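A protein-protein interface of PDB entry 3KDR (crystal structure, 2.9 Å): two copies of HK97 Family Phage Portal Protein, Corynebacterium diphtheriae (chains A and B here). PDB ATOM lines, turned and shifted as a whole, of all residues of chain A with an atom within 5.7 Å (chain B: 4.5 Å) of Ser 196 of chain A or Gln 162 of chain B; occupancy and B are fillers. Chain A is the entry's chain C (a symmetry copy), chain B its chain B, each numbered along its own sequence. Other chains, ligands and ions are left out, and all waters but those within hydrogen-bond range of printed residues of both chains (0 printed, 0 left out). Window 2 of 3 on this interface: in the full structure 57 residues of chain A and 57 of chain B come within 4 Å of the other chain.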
ATOM      1  N   GLN A 162      21.220  -0.099 -30.441  1.00  0.00           N
ATOM      2  CA  GLN A 162      20.985   1.299 -30.161  1.00  0.00           C
ATOM      3  C   GLN A 162      20.048   1.883 -31.169  1.00  0.00           C
ATOM      4  O   GLN A 162      20.183   1.645 -32.359  1.00  0.00           O
ATOM      5  CB  GLN A 162      22.256   2.103 -30.146  1.00  0.00           C
ATOM      6  CG  GLN A 162      22.705   2.499 -28.726  1.00  0.00           C
ATOM      7  CD  GLN A 162      21.651   3.271 -27.875  1.00  0.00           C
ATOM      8  OE1 GLN A 162      21.122   2.730 -26.885  1.00  0.00           O
ATOM      9  NE2 GLN A 162      21.401   4.555 -28.229  1.00  0.00           N
ATOM     10  N   ASN A 164      19.309   5.252 -30.857  1.00  0.00           N
ATOM     11  CA  ASN A 164      19.513   6.654 -30.526  1.00  0.00           C
ATOM     12  C   ASN A 164      20.871   7.098 -30.930  1.00  0.00           C
ATOM     13  O   ASN A 164      21.825   6.321 -30.809  1.00  0.00           O
ATOM     14  CB  ASN A 164      19.552   6.767 -29.018  1.00  0.00           C
ATOM     15  CG  ASN A 164      18.464   7.584 -28.485  1.00  0.00           C
ATOM     16  OD1 ASN A 164      17.354   7.538 -29.013  1.00  0.00           O
ATOM     17  ND2 ASN A 164      18.745   8.336 -27.401  1.00  0.00           N
ATOM     18  N   ALA A 166      22.554   8.831 -29.017  1.00  0.00           N
ATOM     19  CA  ALA A 166      23.158   8.991 -27.666  1.00  0.00           C
ATOM     20  C   ALA A 166      24.665   8.725 -27.622  1.00  0.00           C
ATOM     21  O   ALA A 166      25.146   7.753 -28.171  1.00  0.00           O
ATOM     22  CB  ALA A 166      22.477   8.083 -26.663  1.00  0.00           C
ATOM     23  N   LEU A 168      27.760   7.248 -26.286  1.00  0.00           N
ATOM     24  CA  LEU A 168      28.135   6.219 -25.333  1.00  0.00           C
ATOM     25  C   LEU A 168      29.572   5.827 -25.575  1.00  0.00           C
ATOM     26  O   LEU A 168      29.976   5.479 -26.710  1.00  0.00           O
ATOM     27  CB  LEU A 168      27.261   4.983 -25.466  1.00  0.00           C
ATOM     28  CG  LEU A 168      25.763   5.087 -25.280  1.00  0.00           C
ATOM     29  CD1 LEU A 168      25.112   4.341 -26.508  1.00  0.00           C
ATOM     30  CD2 LEU A 168      25.347   4.561 -23.885  1.00  0.00           C
ATOM     31  N   PHE A 193      19.569  -4.311 -17.432  1.00  0.00           N
ATOM     32  CA  PHE A 193      19.177  -2.943 -17.619  1.00  0.00           C
ATOM     33  C   PHE A 193      19.639  -2.465 -18.988  1.00  0.00           C
ATOM     34  O   PHE A 193      20.764  -2.743 -19.411  1.00  0.00           O
ATOM     35  CB  PHE A 193      19.746  -2.095 -16.493  1.00  0.00           C
ATOM     36  CG  PHE A 193      19.453  -0.659 -16.639  1.00  0.00           C
ATOM     37  CD1 PHE A 193      18.221  -0.169 -16.282  1.00  0.00           C
ATOM     38  CD2 PHE A 193      20.393   0.215 -17.166  1.00  0.00           C
ATOM     39  CE1 PHE A 193      17.932   1.171 -16.415  1.00  0.00           C
ATOM     40  CE2 PHE A 193      20.094   1.543 -17.333  1.00  0.00           C
ATOM     41  CZ  PHE A 193      18.862   2.026 -16.956  1.00  0.00           C
ATOM     42  N   SER A 194      18.753  -1.729 -19.647  1.00  0.00           N
ATOM     43  CA  SER A 194      19.006  -1.107 -20.938  1.00  0.00           C
ATOM     44  C   SER A 194      18.927   0.370 -20.761  1.00  0.00           C
ATOM     45  O   SER A 194      17.857   0.910 -20.528  1.00  0.00           O
ATOM     46  CB  SER A 194      17.947  -1.491 -21.963  1.00  0.00           C
ATOM     47  OG  SER A 194      18.346  -2.658 -22.638  1.00  0.00           O
ATOM     48  N   SER A 195      20.082   1.000 -20.949  1.00  0.00           N
ATOM     49  CA  SER A 195      20.284   2.421 -20.848  1.00  0.00           C
ATOM     50  C   SER A 195      19.492   3.045 -21.964  1.00  0.00           C
ATOM     51  O   SER A 195      18.962   2.377 -22.786  1.00  0.00           O
ATOM     52  CB  SER A 195      21.756   2.746 -21.027  1.00  0.00           C
ATOM     53  OG  SER A 195      21.994   3.080 -22.381  1.00  0.00           O
ATOM     54  N   SER A 196      19.435   4.348 -22.016  1.00  0.00           N
ATOM     55  CA  SER A 196      18.455   4.992 -22.836  1.00  0.00           C
ATOM     56  C   SER A 196      18.713   4.836 -24.299  1.00  0.00           C
ATOM     57  O   SER A 196      19.822   5.029 -24.788  1.00  0.00           O
ATOM     58  CB  SER A 196      18.406   6.463 -22.535  1.00  0.00           C
ATOM     59  OG  SER A 196      17.787   7.122 -23.627  1.00  0.00           O
ATOM     60  N   GLY A 197      17.639   4.495 -24.993  1.00  0.00           N
ATOM     61  CA  GLY A 197      17.642   4.338 -26.435  1.00  0.00           C
ATOM     62  C   GLY A 197      18.075   2.957 -26.899  1.00  0.00           C
ATOM     63  O   GLY A 197      18.002   2.646 -28.094  1.00  0.00           O
ATOM     64  N   LEU A 198      18.535   2.134 -25.955  1.00  0.00           N
ATOM     65  CA  LEU A 198      19.083   0.797 -26.216  1.00  0.00           C
ATOM     66  C   LEU A 198      17.977  -0.172 -26.013  1.00  0.00           C
ATOM     67  O   LEU A 198      17.165   0.025 -25.144  1.00  0.00           O
ATOM     68  CB  LEU A 198      20.179   0.476 -25.223  1.00  0.00           C
ATOM     69  CG  LEU A 198      21.175  -0.557 -25.714  1.00  0.00           C
ATOM     70  CD1 LEU A 198      22.564   0.064 -26.053  1.00  0.00           C
ATOM     71  CD2 LEU A 198      21.295  -1.621 -24.654  1.00  0.00           C
ATOM     72  N   LEU B 160      14.976  -4.030 -18.221  1.00  0.00           N
ATOM     73  CA  LEU B 160      14.428  -2.757 -17.744  1.00  0.00           C
ATOM     74  C   LEU B 160      14.998  -1.697 -18.641  1.00  0.00           C
ATOM     75  O   LEU B 160      16.200  -1.545 -18.737  1.00  0.00           O
ATOM     76  CB  LEU B 160      14.841  -2.485 -16.319  1.00  0.00           C
ATOM     77  CG  LEU B 160      14.571  -3.640 -15.365  1.00  0.00           C
ATOM     78  CD1 LEU B 160      15.200  -3.479 -13.996  1.00  0.00           C
ATOM     79  CD2 LEU B 160      13.118  -3.796 -15.228  1.00  0.00           C
ATOM     80  N   ARG B 161      14.140  -0.950 -19.297  1.00  0.00           N
ATOM     81  CA  ARG B 161      14.528  -0.186 -20.441  1.00  0.00           C
ATOM     82  C   ARG B 161      14.253   1.230 -20.178  1.00  0.00           C
ATOM     83  O   ARG B 161      13.107   1.593 -20.018  1.00  0.00           O
ATOM     84  CB  ARG B 161      13.639  -0.605 -21.587  1.00  0.00           C
ATOM     85  CG  ARG B 161      13.851   0.144 -22.899  1.00  0.00           C
ATOM     86  CD  ARG B 161      14.085  -0.847 -23.970  1.00  0.00           C
ATOM     87  NE  ARG B 161      12.943  -1.101 -24.849  1.00  0.00           N
ATOM     88  CZ  ARG B 161      12.798  -2.207 -25.579  1.00  0.00           C
ATOM     89  NH1 ARG B 161      13.652  -3.221 -25.474  1.00  0.00           N
ATOM     90  NH2 ARG B 161      11.781  -2.318 -26.396  1.00  0.00           N
ATOM     91  N   GLN B 162      15.300   2.041 -20.209  1.00  0.00           N
ATOM     92  CA  GLN B 162      15.217   3.459 -19.934  1.00  0.00           C
ATOM     93  C   GLN B 162      14.788   4.180 -21.198  1.00  0.00           C
ATOM     94  O   GLN B 162      15.255   3.881 -22.252  1.00  0.00           O
ATOM     95  CB  GLN B 162      16.594   3.918 -19.482  1.00  0.00           C
ATOM     96  CG  GLN B 162      16.641   5.305 -18.893  1.00  0.00           C
ATOM     97  CD  GLN B 162      18.068   5.888 -18.808  1.00  0.00           C
ATOM     98  OE1 GLN B 162      18.279   6.929 -18.193  1.00  0.00           O
ATOM     99  NE2 GLN B 162      19.033   5.217 -19.401  1.00  0.00           N
ATOM    100  N   THR B 163      13.858   5.106 -21.109  1.00  0.00           N
ATOM    101  CA  THR B 163      13.416   5.834 -22.322  1.00  0.00           C
ATOM    102  C   THR B 163      13.621   7.336 -22.176  1.00  0.00           C
ATOM    103  O   THR B 163      13.751   8.028 -23.175  1.00  0.00           O
ATOM    104  CB  THR B 163      11.950   5.530 -22.660  1.00  0.00           C
ATOM    105  OG1 THR B 163      11.184   5.480 -21.457  1.00  0.00           O
ATOM    106  CG2 THR B 163      11.859   4.195 -23.318  1.00  0.00           C
ATOM    107  N   ASN B 164      13.637   7.810 -20.920  1.00  0.00           N
ATOM    108  CA  ASN B 164      13.988   9.168 -20.566  1.00  0.00           C
ATOM    109  C   ASN B 164      15.471   9.277 -20.831  1.00  0.00           C
ATOM    110  O   ASN B 164      16.092   8.302 -21.239  1.00  0.00           O
ATOM    111  CB  ASN B 164      13.657   9.448 -19.092  1.00  0.00           C
ATOM    112  CG  ASN B 164      14.781   9.027 -18.120  1.00  0.00           C
ATOM    113  OD1 ASN B 164      15.758   8.388 -18.496  1.00  0.00           O
ATOM    114  ND2 ASN B 164      14.641   9.419 -16.866  1.00  0.00           N
ATOM    115  N   ASN B 165      16.049  10.440 -20.577  1.00  0.00           N
ATOM    116  CA  ASN B 165      17.459  10.646 -20.889  1.00  0.00           C
ATOM    117  C   ASN B 165      18.387  10.911 -19.730  1.00  0.00           C
ATOM    118  O   ASN B 165      19.535  11.263 -19.926  1.00  0.00           O
ATOM    119  CB  ASN B 165      17.578  11.744 -21.935  1.00  0.00           C
ATOM    120  CG  ASN B 165      17.593  11.167 -23.337  1.00  0.00           C
ATOM    121  OD1 ASN B 165      18.632  10.647 -23.789  1.00  0.00           O
ATOM    122  ND2 ASN B 165      16.437  11.194 -24.011  1.00  0.00           N
ATOM    123  N   ALA B 166      17.882  10.708 -18.528  1.00  0.00           N
ATOM    124  CA  ALA B 166      18.697  10.800 -17.337  1.00  0.00           C
ATOM    125  C   ALA B 166      19.925   9.914 -17.465  1.00  0.00           C
ATOM    126  O   ALA B 166      19.852   8.836 -18.033  1.00  0.00           O
ATOM    127  CB  ALA B 166      17.891  10.378 -16.142  1.00  0.00           C
ATOM    128  N   LEU B 168      22.394   7.625 -15.349  1.00  0.00           N
ATOM    129  CA  LEU B 168      22.328   6.955 -14.063  1.00  0.00           C
ATOM    130  C   LEU B 168      23.627   6.267 -13.783  1.00  0.00           C
ATOM    131  O   LEU B 168      24.224   5.657 -14.653  1.00  0.00           O
ATOM    132  CB  LEU B 168      21.228   5.904 -13.987  1.00  0.00           C
ATOM    133  CG  LEU B 168      19.885   6.170 -14.629  1.00  0.00           C
ATOM    134  CD1 LEU B 168      19.300   4.837 -14.934  1.00  0.00           C
ATOM    135  CD2 LEU B 168      18.980   6.929 -13.692  1.00  0.00           C
ATOM    136  N   LEU B 198      10.802   4.185 -17.558  1.00  0.00           N
ATOM    137  CA  LEU B 198      11.234   2.823 -17.710  1.00  0.00           C
ATOM    138  C   LEU B 198      10.141   1.917 -18.116  1.00  0.00           C
ATOM    139  O   LEU B 198       9.049   2.089 -17.709  1.00  0.00           O
ATOM    140  CB  LEU B 198      11.804   2.343 -16.419  1.00  0.00           C
ATOM    141  CG  LEU B 198      12.790   1.222 -16.520  1.00  0.00           C
ATOM    142  CD1 LEU B 198      14.139   1.767 -16.396  1.00  0.00           C
ATOM    143  CD2 LEU B 198      12.522   0.293 -15.446  1.00  0.00           C
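The backbone NH (N) of Ser 194 of chain A is in hydrogen-bond range of the backbone carbonyl oxygen (O) of Leu 160 of chain B, 2.7 Å away. The backbone carbonyl oxygen (O) of Ser 194 of chain A lies within hydrogen-bond range of the backbone NH (N) of Gln 162 of chain B, at 2.8 Å. The side-chain amide nitrogen (NE2) of Gln 162 of chain B lies close to the backbone NH (N) of Ser 196 of chain A, 2.8 Å away. The backbone carbonyl oxygen (O) of Asn 164 of chain B sits at hydrogen-bond distance from the side-chain hydroxyl (OG) of Ser 196 of chain A (3.2 Å).
The side-chain amide oxygen (OE1) of Gln 162 of chain B lies close to the side-chain amide oxygen (OD1) of Asn 164 of chain B (2.9 Å). The side-chain amide oxygen (OE1) of Gln 162 of chain B sits close to the backbone carbonyl oxygen (O) of Ala 166 of chain B, at 2.5 Å. N of Ala 166 of chain B is in hydrogen-bond range of OD1 of Asn 164 of chain B, at 3.1 Å. OE1 of Gln 162 of chain A sits close to O of Ser 196 of chain A, 3.4 Å away. The side-chain amide oxygen of Gln 162 of chain A lies close to the backbone carbonyl oxygen of Gly 197 of chain A (3.3 Å). The side-chain amide oxygen (OE1) of Gln 162 of chain A is in hydrogen-bond range of the backbone NH (N) of Leu 198 of chain A (2.8 Å).
Leu 160 of chain B touches Phe 193 of chain A. Gln 162 of chain B touches Phe 193 of chain A (CB to CZ, 3.9 Å). CD1 of Leu 168 of chain B touches CZ of Phe 193 of chain A, 3.5 Å away. Phe 193 of chain A touches Leu 198 of chain B. O of Ser 194 of chain A touches CA of Arg 161 of chain B, 3.5 Å away. Gln 162 of chain B touches Ser 195 of chain A. OD1 of Asn 165 of chain B touches OG of Ser 196 of chain A (3.6 Å). O of Gln 162 of chain B touches N of Gly 197 of chain A (3.7 Å). Leu 198 of chain A touches Arg 161 of chain B.
Of the printed residues of chain B, Ser 196 of chain A touches Gln 162 (2.8 Å), Asn 164 (3.2 Å) and Asn 165 (3.6 Å). Gln 162 of chain B touches just these residues of chain A: Phe 193 (3.9 Å), Ser 194 (2.8 Å), Ser 195 (3.4 Å), Ser 196 (2.8 Å) and Gly 197 (3.7 Å). Of the printed residues of chain A, Leu 160 of chain B touches Phe 193 and Ser 194. Of the printed residues of chain B, Phe 193 of chain A touches Leu 160, Gln 162, Leu 168 and Leu 198. Of the printed residues of chain B, Ser 195 of chain A touches Gln 162 (3.4 Å). Of the printed residues of chain A, Asn 164 of chain B touches Ser 196 (3.2 Å). Of the printed residues of chain A, Asn 165 of chain B touches Ser 196. Ala 166 of chain B touches none of the printed residues of chain A. Gln 162 of chain A touches none of the printed residues of chain B. The nearest residue of chain B that does not touch Ser 196 of chain A is Thr 163 of chain B (4.2 Å). The nearest residue of chain A that does not touch Gln 162 of chain B is Leu 198 of chain A (5.2 Å).
Hydrophobic or aromatic side chains of chain B that line the printed part of chain A: Leu 168 and Leu 198. Of the 10 printed residues of chain A, 6 touch a printed residue of chain B. Hydrophobic or aromatic side chains of chain A within 4 Å of the printed part of chain B: Phe 193. Among the printed residues, no Asp or Glu carboxylate lies within 4 Å of a Lys or Arg side-chain nitrogen of the other chain.
Positions printed for both chains: 162, 164, 166, 168 and 198. Of the 13 pairs that touch across the chains among the printed residues, none has its exchanged pair printed and touching as well.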
